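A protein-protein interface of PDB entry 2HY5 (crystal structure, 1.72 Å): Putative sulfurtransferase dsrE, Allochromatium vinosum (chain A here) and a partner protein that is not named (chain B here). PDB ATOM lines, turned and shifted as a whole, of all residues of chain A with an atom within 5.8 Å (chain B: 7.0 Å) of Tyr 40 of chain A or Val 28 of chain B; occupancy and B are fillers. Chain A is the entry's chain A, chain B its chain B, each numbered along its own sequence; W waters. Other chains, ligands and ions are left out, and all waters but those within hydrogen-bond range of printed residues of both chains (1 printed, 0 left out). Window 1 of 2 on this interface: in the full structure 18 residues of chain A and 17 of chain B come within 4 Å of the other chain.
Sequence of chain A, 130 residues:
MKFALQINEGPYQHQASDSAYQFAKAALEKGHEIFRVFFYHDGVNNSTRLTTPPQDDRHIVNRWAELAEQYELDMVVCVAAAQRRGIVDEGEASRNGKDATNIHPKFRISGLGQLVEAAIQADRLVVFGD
Tyr 40 of chain A touches three residues of chain B.
Val 28 of chain B touches just these residues of chain A: Tyr 40 (3.7 Å) and Leu 112 (3.6 Å).
Of the printed residues of chain B, Ala 81 of chain A touches Glu 24.
Of the printed residues of chain A, Glu 24 of chain B touches Tyr 40, His 41 and Ala 81.
Val 44 of chain A touches none of the printed residues of chain B.
The nearest residue of chain A that does not touch Val 28 of chain B is Val 116 of chain A (4.3 Å).
The nearest printed residue of chain A that does not touch Glu 27 of chain B is Ala 80 of chain A (5.1 Å).
The side-chain amide nitrogen of Asn 8 of chain A lies within hydrogen-bond range of the backbone carbonyl oxygen of Ser 135 of chain B, at 3.5 Å.
OH of Tyr 21 of chain B sits at hydrogen-bond distance from OE2 of Glu 9 of chain A, 2.6 Å away.
OH of Tyr 40 of chain A sits at hydrogen-bond distance from O of Glu 24 of chain B (2.7 Å).
ND1 of His 41 of chain A lies within hydrogen-bond range of OE1 of Glu 24 of chain B (2.6 Å).
Phe 134 of chain B touches Gln 6 of chain A (CD1 to OE1, 3.9 Å).
Gln 6 of chain A touches Ser 135 of chain B.
OH of Tyr 40 of chain A touches CB of Glu 27 of chain B (3.6 Å).
CE2 of Tyr 40 of chain A touches CG2 of Val 28 of chain B (3.7 Å).
His 41 of chain A touches Tyr 21 of chain B (NE2 to CD2, 3.9 Å).
His 41 of chain A touches Phe 136 of chain B (NE2 to CD2, 3.5 Å).
Ala 81 of chain A touches Glu 24 of chain B (CB to OE2, 3.9 Å).
Glu 27 of chain B touches Leu 112 of chain A.
CD2 of Leu 112 of chain A touches CG2 of Val 28 of chain B (3.6 Å).
Ile 31 of chain B touches Leu 112 of chain A (CG1 to CD2, 3.9 Å).
Water W1 lies within hydrogen-bond range of the side-chain carboxylate of Glu 9 of chain A (2.8 Å), the chain-end carboxylate of Phe 136 of chain B (2.9 Å) and the side-chain amide nitrogen of Asn 8 of chain A (3.5 Å).
The side-chain amide nitrogen (NE2) of Gln 6 of chain A is in hydrogen-bond range of the side-chain amide oxygen (OD1) of Asn 8 of chain A (2.8 Å).
The backbone carbonyl oxygen (O) of Ile 7 of chain A sits at hydrogen-bond distance from the backbone NH (N) of Tyr 40 of chain A, at 3.0 Å.
The backbone carbonyl oxygen (O) of Asn 8 of chain A is in hydrogen-bond range of the backbone NH (N) of Asp 42 of chain A, at 3.4 Å.
N of Gly 43 of chain A is in hydrogen-bond range of O of Asn 8 of chain A, at 3.4 Å.
SG of Cys 78 of chain A is in hydrogen-bond range of N of Ala 81 of chain A, at 3.6 Å.
Printed residues of chain A that touch a printed residue of chain B: Gln 6, Asn 8, Glu 9, Tyr 40, His 41, Ala 81, Leu 112 and Val 116.
Among the printed residues, 15 pairs touch across the chains.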
ATOM      1  N   GLN A   6      17.784  15.825  -5.541  1.00  0.00           N
ATOM      2  CA  GLN A   6      18.872  15.189  -4.816  1.00  0.00           C
ATOM      3  C   GLN A   6      18.663  15.465  -3.330  1.00  0.00           C
ATOM      4  O   GLN A   6      18.435  16.610  -2.941  1.00  0.00           O
ATOM      5  CB  GLN A   6      20.213  15.775  -5.276  1.00  0.00           C
ATOM      6  CG  GLN A   6      21.442  15.040  -4.746  1.00  0.00           C
ATOM      7  CD  GLN A   6      22.735  15.765  -5.092  1.00  0.00           C
ATOM      8  OE1 GLN A   6      22.896  16.280  -6.200  1.00  0.00           O
ATOM      9  NE2 GLN A   6      23.680  15.771  -4.154  1.00  0.00           N
ATOM     10  N   ILE A   7      18.721  14.416  -2.513  1.00  0.00           N
ATOM     11  CA  ILE A   7      18.545  14.544  -1.067  1.00  0.00           C
ATOM     12  C   ILE A   7      19.815  14.010  -0.409  1.00  0.00           C
ATOM     13  O   ILE A   7      20.176  12.850  -0.602  1.00  0.00           O
ATOM     14  CB  ILE A   7      17.302  13.755  -0.603  1.00  0.00           C
ATOM     15  CG1 ILE A   7      16.057  14.331  -1.295  1.00  0.00           C
ATOM     16  CG2 ILE A   7      17.146  13.844   0.914  1.00  0.00           C
ATOM     17  CD1 ILE A   7      14.802  13.536  -1.084  1.00  0.00           C
ATOM     18  N   ASN A   8      20.484  14.864   0.368  1.00  0.00           N
ATOM     19  CA  ASN A   8      21.757  14.512   0.998  1.00  0.00           C
ATOM     20  C   ASN A   8      21.765  14.167   2.476  1.00  0.00           C
ATOM     21  O   ASN A   8      22.821  13.833   3.018  1.00  0.00           O
ATOM     22  CB  ASN A   8      22.768  15.646   0.812  1.00  0.00           C
ATOM     23  CG  ASN A   8      22.944  16.052  -0.636  1.00  0.00           C
ATOM     24  OD1 ASN A   8      22.802  15.238  -1.545  1.00  0.00           O
ATOM     25  ND2 ASN A   8      23.288  17.313  -0.851  1.00  0.00           N
ATOM     26  N   GLU A   9      20.620  14.249   3.136  1.00  0.00           N
ATOM     27  CA  GLU A   9      20.588  13.969   4.563  1.00  0.00           C
ATOM     28  C   GLU A   9      19.610  12.887   4.958  1.00  0.00           C
ATOM     29  O   GLU A   9      18.624  12.638   4.265  1.00  0.00           O
ATOM     30  CB  GLU A   9      20.251  15.247   5.327  1.00  0.00           C
ATOM     31  CG  GLU A   9      21.133  16.422   4.969  1.00  0.00           C
ATOM     32  CD  GLU A   9      22.611  16.129   5.154  1.00  0.00           C
ATOM     33  OE1 GLU A   9      22.955  15.369   6.083  1.00  0.00           O
ATOM     34  OE2 GLU A   9      23.427  16.677   4.380  1.00  0.00           O
ATOM     35  N   PHE A  38      17.083  11.204  -6.240  1.00  0.00           N
ATOM     36  CA  PHE A  38      18.332  10.538  -5.917  1.00  0.00           C
ATOM     37  C   PHE A  38      18.799  10.816  -4.494  1.00  0.00           C
ATOM     38  O   PHE A  38      18.924  11.969  -4.090  1.00  0.00           O
ATOM     39  CB  PHE A  38      19.406  10.970  -6.918  1.00  0.00           C
ATOM     40  CG  PHE A  38      20.642  10.127  -6.880  1.00  0.00           C
ATOM     41  CD1 PHE A  38      21.632  10.358  -5.932  1.00  0.00           C
ATOM     42  CD2 PHE A  38      20.802   9.075  -7.775  1.00  0.00           C
ATOM     43  CE1 PHE A  38      22.766   9.553  -5.875  1.00  0.00           C
ATOM     44  CE2 PHE A  38      21.930   8.260  -7.730  1.00  0.00           C
ATOM     45  CZ  PHE A  38      22.915   8.498  -6.777  1.00  0.00           C
ATOM     46  N   PHE A  39      19.038   9.749  -3.738  1.00  0.00           N
ATOM     47  CA  PHE A  39      19.495   9.883  -2.361  1.00  0.00           C
ATOM     48  C   PHE A  39      20.992   9.630  -2.282  1.00  0.00           C
ATOM     49  O   PHE A  39      21.479   8.576  -2.700  1.00  0.00           O
ATOM     50  CB  PHE A  39      18.735   8.916  -1.450  1.00  0.00           C
ATOM     51  CG  PHE A  39      17.250   9.147  -1.432  1.00  0.00           C
ATOM     52  CD1 PHE A  39      16.425   8.548  -2.377  1.00  0.00           C
ATOM     53  CD2 PHE A  39      16.681   9.993  -0.492  1.00  0.00           C
ATOM     54  CE1 PHE A  39      15.049   8.786  -2.381  1.00  0.00           C
ATOM     55  CE2 PHE A  39      15.309  10.236  -0.487  1.00  0.00           C
ATOM     56  CZ  PHE A  39      14.495   9.634  -1.435  1.00  0.00           C
ATOM     57  N   TYR A  40      21.719  10.610  -1.751  1.00  0.00           N
ATOM     58  CA  TYR A  40      23.171  10.531  -1.631  1.00  0.00           C
ATOM     59  C   TYR A  40      23.598  10.873  -0.201  1.00  0.00           C
ATOM     60  O   TYR A  40      22.799  11.394   0.574  1.00  0.00           O
ATOM     61  CB  TYR A  40      23.823  11.497  -2.627  1.00  0.00           C
ATOM     62  CG  TYR A  40      25.287  11.231  -2.878  1.00  0.00           C
ATOM     63  CD1 TYR A  40      25.759   9.926  -3.038  1.00  0.00           C
ATOM     64  CD2 TYR A  40      26.201  12.280  -2.982  1.00  0.00           C
ATOM     65  CE1 TYR A  40      27.102   9.673  -3.293  1.00  0.00           C
ATOM     66  CE2 TYR A  40      27.548  12.035  -3.241  1.00  0.00           C
ATOM     67  CZ  TYR A  40      27.992  10.731  -3.394  1.00  0.00           C
ATOM     68  OH  TYR A  40      29.320  10.471  -3.652  1.00  0.00           O
ATOM     69  N   HIS A  41      24.854  10.595   0.141  1.00  0.00           N
ATOM     70  CA  HIS A  41      25.354  10.844   1.498  1.00  0.00           C
ATOM     71  C   HIS A  41      24.397  10.138   2.470  1.00  0.00           C
ATOM     72  O   HIS A  41      23.875   9.069   2.157  1.00  0.00           O
ATOM     73  CB  HIS A  41      25.385  12.347   1.815  1.00  0.00           C
ATOM     74  CG  HIS A  41      26.172  13.170   0.840  1.00  0.00           C
ATOM     75  ND1 HIS A  41      27.518  12.979   0.608  1.00  0.00           N
ATOM     76  CD2 HIS A  41      25.808  14.223   0.068  1.00  0.00           C
ATOM     77  CE1 HIS A  41      27.948  13.875  -0.260  1.00  0.00           C
ATOM     78  NE2 HIS A  41      26.929  14.644  -0.604  1.00  0.00           N
ATOM     79  N   ASP A  42      24.161  10.732   3.639  1.00  0.00           N
ATOM     80  CA  ASP A  42      23.244  10.147   4.621  1.00  0.00           C
ATOM     81  C   ASP A  42      21.826  10.057   4.062  1.00  0.00           C
ATOM     82  O   ASP A  42      20.947   9.444   4.666  1.00  0.00           O
ATOM     83  CB  ASP A  42      23.229  10.975   5.909  1.00  0.00           C
ATOM     84  CG  ASP A  42      24.251  10.502   6.924  1.00  0.00           C
ATOM     85  OD1 ASP A  42      25.008   9.554   6.619  1.00  0.00           O
ATOM     86  OD2 ASP A  42      24.294  11.080   8.032  1.00  0.00           O
ATOM     87  N   GLY A  43      21.610  10.675   2.905  1.00  0.00           N
ATOM     88  CA  GLY A  43      20.304  10.634   2.277  1.00  0.00           C
ATOM     89  C   GLY A  43      19.864   9.211   1.990  1.00  0.00           C
ATOM     90  O   GLY A  43      18.668   8.926   1.942  1.00  0.00           O
ATOM     91  N   VAL A  44      20.819   8.307   1.802  1.00  0.00           N
ATOM     92  CA  VAL A  44      20.467   6.919   1.517  1.00  0.00           C
ATOM     93  C   VAL A  44      19.643   6.288   2.641  1.00  0.00           C
ATOM     94  O   VAL A  44      18.921   5.314   2.416  1.00  0.00           O
ATOM     95  CB  VAL A  44      21.730   6.049   1.267  1.00  0.00           C
ATOM     96  CG1 VAL A  44      22.514   6.606   0.081  1.00  0.00           C
ATOM     97  CG2 VAL A  44      22.597   6.013   2.517  1.00  0.00           C
ATOM     98  N   VAL A  76      16.115   6.478  -6.416  1.00  0.00           N
ATOM     99  CA  VAL A  76      17.398   5.802  -6.475  1.00  0.00           C
ATOM    100  C   VAL A  76      18.300   6.122  -5.293  1.00  0.00           C
ATOM    101  O   VAL A  76      18.413   7.276  -4.866  1.00  0.00           O
ATOM    102  CB  VAL A  76      18.127   6.170  -7.788  1.00  0.00           C
ATOM    103  CG1 VAL A  76      19.385   5.322  -7.961  1.00  0.00           C
ATOM    104  CG2 VAL A  76      17.177   5.979  -8.968  1.00  0.00           C
ATOM    105  N   CYS A  78      22.219   5.728  -3.874  1.00  0.00           N
ATOM    106  CA  CYS A  78      23.603   5.510  -4.283  1.00  0.00           C
ATOM    107  C   CYS A  78      24.202   4.265  -3.631  1.00  0.00           C
ATOM    108  O   CYS A  78      24.202   4.136  -2.407  1.00  0.00           O
ATOM    109  CB  CYS A  78      24.458   6.720  -3.918  1.00  0.00           C
ATOM    110  SG  CYS A  78      26.195   6.503  -4.335  1.00  0.00           S
ATOM    111  N   ALA A  80      27.417   3.268  -3.457  1.00  0.00           N
ATOM    112  CA  ALA A  80      28.632   3.570  -2.702  1.00  0.00           C
ATOM    113  C   ALA A  80      28.293   4.107  -1.319  1.00  0.00           C
ATOM    114  O   ALA A  80      28.823   3.639  -0.307  1.00  0.00           O
ATOM    115  CB  ALA A  80      29.478   4.584  -3.464  1.00  0.00           C
ATOM    116  N   ALA A  81      27.406   5.094  -1.282  1.00  0.00           N
ATOM    117  CA  ALA A  81      26.981   5.692  -0.026  1.00  0.00           C
ATOM    118  C   ALA A  81      26.194   4.680   0.812  1.00  0.00           C
ATOM    119  O   ALA A  81      26.269   4.686   2.037  1.00  0.00           O
ATOM    120  CB  ALA A  81      26.130   6.933  -0.302  1.00  0.00           C
ATOM    121  N   LEU A 112      26.096   6.092  -8.980  1.00  0.00           N
ATOM    122  CA  LEU A 112      26.078   7.540  -8.885  1.00  0.00           C
ATOM    123  C   LEU A 112      25.823   8.143 -10.265  1.00  0.00           C
ATOM    124  O   LEU A 112      25.355   9.279 -10.385  1.00  0.00           O
ATOM    125  CB  LEU A 112      27.419   8.025  -8.321  1.00  0.00           C
ATOM    126  CG  LEU A 112      27.517   9.423  -7.708  1.00  0.00           C
ATOM    127  CD1 LEU A 112      26.398   9.635  -6.702  1.00  0.00           C
ATOM    128  CD2 LEU A 112      28.881   9.574  -7.030  1.00  0.00           C
ATOM    129  N   LEU A 115      22.588   9.817 -11.027  1.00  0.00           N
ATOM    130  CA  LEU A 115      22.369  11.187 -10.574  1.00  0.00           C
ATOM    131  C   LEU A 115      22.779  12.143 -11.691  1.00  0.00           C
ATOM    132  O   LEU A 115      22.025  13.036 -12.077  1.00  0.00           O
ATOM    133  CB  LEU A 115      23.202  11.487  -9.323  1.00  0.00           C
ATOM    134  CG  LEU A 115      23.231  12.962  -8.897  1.00  0.00           C
ATOM    135  CD1 LEU A 115      21.832  13.420  -8.525  1.00  0.00           C
ATOM    136  CD2 LEU A 115      24.186  13.141  -7.723  1.00  0.00           C
ATOM    137  N   VAL A 116      23.988  11.950 -12.208  1.00  0.00           N
ATOM    138  CA  VAL A 116      24.486  12.796 -13.284  1.00  0.00           C
ATOM    139  C   VAL A 116      23.562  12.663 -14.488  1.00  0.00           C
ATOM    140  O   VAL A 116      23.232  13.650 -15.146  1.00  0.00           O
ATOM    141  CB  VAL A 116      25.917  12.389 -13.683  1.00  0.00           C
ATOM    142  CG1 VAL A 116      26.405  13.257 -14.833  1.00  0.00           C
ATOM    143  CG2 VAL A 116      26.844  12.530 -12.476  1.00  0.00           C
ATOM    144  N   TYR B  10      30.309  22.215  -9.910  1.00  0.00           N
ATOM    145  CA  TYR B  10      30.394  21.460  -8.666  1.00  0.00           C
ATOM    146  C   TYR B  10      30.840  22.473  -7.628  1.00  0.00           C
ATOM    147  O   TYR B  10      31.990  22.901  -7.634  1.00  0.00           O
ATOM    148  CB  TYR B  10      31.424  20.340  -8.803  1.00  0.00           C
ATOM    149  CG  TYR B  10      30.946  19.224  -9.695  1.00  0.00           C
ATOM    150  CD1 TYR B  10      30.184  18.179  -9.179  1.00  0.00           C
ATOM    151  CD2 TYR B  10      31.224  19.226 -11.063  1.00  0.00           C
ATOM    152  CE1 TYR B  10      29.708  17.161  -9.998  1.00  0.00           C
ATOM    153  CE2 TYR B  10      30.748  18.209 -11.894  1.00  0.00           C
ATOM    154  CZ  TYR B  10      29.992  17.180 -11.351  1.00  0.00           C
ATOM    155  OH  TYR B  10      29.513  16.170 -12.157  1.00  0.00           O
ATOM    156  N   TYR B  21      31.267  15.358   3.047  1.00  0.00           N
ATOM    157  CA  TYR B  21      30.923  16.093   1.832  1.00  0.00           C
ATOM    158  C   TYR B  21      32.053  16.298   0.822  1.00  0.00           C
ATOM    159  O   TYR B  21      31.831  16.175  -0.380  1.00  0.00           O
ATOM    160  CB  TYR B  21      30.294  17.444   2.192  1.00  0.00           C
ATOM    161  CG  TYR B  21      29.065  17.303   3.069  1.00  0.00           C
ATOM    162  CD1 TYR B  21      29.097  17.674   4.412  1.00  0.00           C
ATOM    163  CD2 TYR B  21      27.886  16.754   2.568  1.00  0.00           C
ATOM    164  CE1 TYR B  21      27.989  17.503   5.238  1.00  0.00           C
ATOM    165  CE2 TYR B  21      26.766  16.575   3.388  1.00  0.00           C
ATOM    166  CZ  TYR B  21      26.827  16.953   4.722  1.00  0.00           C
ATOM    167  OH  TYR B  21      25.737  16.775   5.548  1.00  0.00           O
ATOM    168  N   TRP B  23      34.814  14.432   0.283  1.00  0.00           N
ATOM    169  CA  TRP B  23      35.141  13.169  -0.369  1.00  0.00           C
ATOM    170  C   TRP B  23      34.030  12.646  -1.275  1.00  0.00           C
ATOM    171  O   TRP B  23      34.283  12.270  -2.420  1.00  0.00           O
ATOM    172  CB  TRP B  23      35.489  12.107   0.679  1.00  0.00           C
ATOM    173  CG  TRP B  23      35.640  10.733   0.099  1.00  0.00           C
ATOM    174  CD1 TRP B  23      34.981   9.604   0.491  1.00  0.00           C
ATOM    175  CD2 TRP B  23      36.473  10.350  -1.001  1.00  0.00           C
ATOM    176  NE1 TRP B  23      35.348   8.540  -0.298  1.00  0.00           N
ATOM    177  CE2 TRP B  23      36.267   8.970  -1.225  1.00  0.00           C
ATOM    178  CE3 TRP B  23      37.377  11.037  -1.824  1.00  0.00           C
ATOM    179  CZ2 TRP B  23      36.924   8.263  -2.234  1.00  0.00           C
ATOM    180  CZ3 TRP B  23      38.033  10.333  -2.832  1.00  0.00           C
ATOM    181  CH2 TRP B  23      37.802   8.961  -3.025  1.00  0.00           C
ATOM    182  N   GLU B  24      32.797  12.621  -0.783  1.00  0.00           N
ATOM    183  CA  GLU B  24      31.721  12.110  -1.618  1.00  0.00           C
ATOM    184  C   GLU B  24      31.386  13.054  -2.767  1.00  0.00           C
ATOM    185  O   GLU B  24      30.868  12.621  -3.792  1.00  0.00           O
ATOM    186  CB  GLU B  24      30.490  11.760  -0.764  1.00  0.00           C
ATOM    187  CG  GLU B  24      30.749  10.533   0.118  1.00  0.00           C
ATOM    188  CD  GLU B  24      29.515   9.994   0.819  1.00  0.00           C
ATOM    189  OE1 GLU B  24      28.711  10.799   1.334  1.00  0.00           O
ATOM    190  OE2 GLU B  24      29.359   8.754   0.866  1.00  0.00           O
ATOM    191  N   ALA B  25      31.710  14.335  -2.614  1.00  0.00           N
ATOM    192  CA  ALA B  25      31.476  15.295  -3.690  1.00  0.00           C
ATOM    193  C   ALA B  25      32.486  14.974  -4.794  1.00  0.00           C
ATOM    194  O   ALA B  25      32.148  14.957  -5.976  1.00  0.00           O
ATOM    195  CB  ALA B  25      31.684  16.718  -3.195  1.00  0.00           C
ATOM    196  N   LEU B  26      33.731  14.724  -4.393  1.00  0.00           N
ATOM    197  CA  LEU B  26      34.794  14.396  -5.338  1.00  0.00           C
ATOM    198  C   LEU B  26      34.411  13.147  -6.132  1.00  0.00           C
ATOM    199  O   LEU B  26      34.716  13.033  -7.319  1.00  0.00           O
ATOM    200  CB  LEU B  26      36.111  14.175  -4.583  1.00  0.00           C
ATOM    201  CG  LEU B  26      37.386  13.934  -5.395  1.00  0.00           C
ATOM    202  CD1 LEU B  26      37.573  15.041  -6.420  1.00  0.00           C
ATOM    203  CD2 LEU B  26      38.581  13.877  -4.444  1.00  0.00           C
ATOM    204  N   GLU B  27      33.731  12.215  -5.470  1.00  0.00           N
ATOM    205  CA  GLU B  27      33.288  10.982  -6.118  1.00  0.00           C
ATOM    206  C   GLU B  27      32.357  11.276  -7.297  1.00  0.00           C
ATOM    207  O   GLU B  27      32.422  10.606  -8.331  1.00  0.00           O
ATOM    208  CB  GLU B  27      32.561  10.085  -5.109  1.00  0.00           C
ATOM    209  CG  GLU B  27      33.464   9.369  -4.124  1.00  0.00           C
ATOM    210  CD  GLU B  27      34.096   8.122  -4.711  1.00  0.00           C
ATOM    211  OE1 GLU B  27      33.917   7.034  -4.120  1.00  0.00           O
ATOM    212  OE2 GLU B  27      34.771   8.226  -5.761  1.00  0.00           O
ATOM    213  N   VAL B  28      31.498  12.282  -7.145  1.00  0.00           N
ATOM    214  CA  VAL B  28      30.560  12.649  -8.204  1.00  0.00           C
ATOM    215  C   VAL B  28      31.294  13.226  -9.413  1.00  0.00           C
ATOM    216  O   VAL B  28      30.943  12.939 -10.559  1.00  0.00           O
ATOM    217  CB  VAL B  28      29.525  13.690  -7.713  1.00  0.00           C
ATOM    218  CG1 VAL B  28      28.533  13.999  -8.835  1.00  0.00           C
ATOM    219  CG2 VAL B  28      28.775  13.153  -6.499  1.00  0.00           C
ATOM    220  N   VAL B  29      32.313  14.040  -9.159  1.00  0.00           N
ATOM    221  CA  VAL B  29      33.075  14.635 -10.249  1.00  0.00           C
ATOM    222  C   VAL B  29      33.720  13.549 -11.100  1.00  0.00           C
ATOM    223  O   VAL B  29      33.689  13.620 -12.327  1.00  0.00           O
ATOM    224  CB  VAL B  29      34.176  15.581  -9.720  1.00  0.00           C
ATOM    225  CG1 VAL B  29      35.015  16.109 -10.878  1.00  0.00           C
ATOM    226  CG2 VAL B  29      33.545  16.728  -8.958  1.00  0.00           C
ATOM    227  N   LEU B  30      34.293  12.537 -10.450  1.00  0.00           N
ATOM    228  CA  LEU B  30      34.951  11.448 -11.169  1.00  0.00           C
ATOM    229  C   LEU B  30      33.936  10.675 -12.007  1.00  0.00           C
ATOM    230  O   LEU B  30      34.201  10.329 -13.159  1.00  0.00           O
ATOM    231  CB  LEU B  30      35.642  10.499 -10.185  1.00  0.00           C
ATOM    232  CG  LEU B  30      36.691  11.123  -9.255  1.00  0.00           C
ATOM    233  CD1 LEU B  30      37.313  10.034  -8.383  1.00  0.00           C
ATOM    234  CD2 LEU B  30      37.757  11.825 -10.073  1.00  0.00           C
ATOM    235  N   ILE B  31      32.773  10.412 -11.423  1.00  0.00           N
ATOM    236  CA  ILE B  31      31.711   9.692 -12.118  1.00  0.00           C
ATOM    237  C   ILE B  31      31.176  10.500 -13.301  1.00  0.00           C
ATOM    238  O   ILE B  31      30.949   9.964 -14.386  1.00  0.00           O
ATOM    239  CB  ILE B  31      30.538   9.381 -11.154  1.00  0.00           C
ATOM    240  CG1 ILE B  31      30.969   8.327 -10.133  1.00  0.00           C
ATOM    241  CG2 ILE B  31      29.313   8.921 -11.937  1.00  0.00           C
ATOM    242  CD1 ILE B  31      31.250   6.960 -10.732  1.00  0.00           C
ATOM    243  N   GLY B  32      30.986  11.796 -13.086  1.00  0.00           N
ATOM    244  CA  GLY B  32      30.464  12.653 -14.137  1.00  0.00           C
ATOM    245  C   GLY B  32      31.370  12.799 -15.345  1.00  0.00           C
ATOM    246  O   GLY B  32      30.920  13.201 -16.419  1.00  0.00           O
ATOM    247  N   ALA B  33      32.646  12.471 -15.178  1.00  0.00           N
ATOM    248  CA  ALA B  33      33.609  12.585 -16.265  1.00  0.00           C
ATOM    249  C   ALA B  33      33.199  11.814 -17.516  1.00  0.00           C
ATOM    250  O   ALA B  33      33.338  12.315 -18.636  1.00  0.00           O
ATOM    251  CB  ALA B  33      34.983  12.113 -15.796  1.00  0.00           C
ATOM    252  N   PHE B 134      25.729  21.249  -8.616  1.00  0.00           N
ATOM    253  CA  PHE B 134      25.770  20.175  -7.640  1.00  0.00           C
ATOM    254  C   PHE B 134      26.285  20.784  -6.347  1.00  0.00           C
ATOM    255  O   PHE B 134      27.371  21.358  -6.318  1.00  0.00           O
ATOM    256  CB  PHE B 134      26.725  19.078  -8.103  1.00  0.00           C
ATOM    257  CG  PHE B 134      26.206  18.274  -9.258  1.00  0.00           C
ATOM    258  CD1 PHE B 134      25.364  17.191  -9.039  1.00  0.00           C
ATOM    259  CD2 PHE B 134      26.548  18.607 -10.565  1.00  0.00           C
ATOM    260  CE1 PHE B 134      24.869  16.446 -10.103  1.00  0.00           C
ATOM    261  CE2 PHE B 134      26.057  17.867 -11.639  1.00  0.00           C
ATOM    262  CZ  PHE B 134      25.216  16.784 -11.408  1.00  0.00           C
ATOM    263  N   SER B 135      25.491  20.670  -5.290  1.00  0.00           N
ATOM    264  CA  SER B 135      25.864  21.190  -3.981  1.00  0.00           C
ATOM    265  C   SER B 135      25.980  20.029  -3.005  1.00  0.00           C
ATOM    266  O   SER B 135      25.255  19.040  -3.117  1.00  0.00           O
ATOM    267  CB  SER B 135      24.814  22.181  -3.484  1.00  0.00           C
ATOM    268  OG  SER B 135      24.707  23.281  -4.373  1.00  0.00           O
ATOM    269  N   PHE B 136      26.898  20.153  -2.051  1.00  0.00           N
ATOM    270  CA  PHE B 136      27.117  19.105  -1.061  1.00  0.00           C
ATOM    271  C   PHE B 136      27.404  19.720   0.303  1.00  0.00           C
ATOM    272  O   PHE B 136      28.493  20.308   0.462  1.00  0.00           O
ATOM    273  CB  PHE B 136      28.297  18.213  -1.467  1.00  0.00           C
ATOM    274  CG  PHE B 136      28.317  17.852  -2.925  1.00  0.00           C
ATOM    275  CD1 PHE B 136      28.822  18.745  -3.865  1.00  0.00           C
ATOM    276  CD2 PHE B 136      27.838  16.620  -3.359  1.00  0.00           C
ATOM    277  CE1 PHE B 136      28.852  18.419  -5.213  1.00  0.00           C
ATOM    278  CE2 PHE B 136      27.864  16.283  -4.709  1.00  0.00           C
ATOM    279  CZ  PHE B 136      28.373  17.186  -5.637  1.00  0.00           C
ATOM    280  OXT PHE B 136      26.543  19.614   1.200  1.00  0.00           O
HETATM  281  O   HOH W   1      24.224  18.337   2.337  1.00  0.00           O
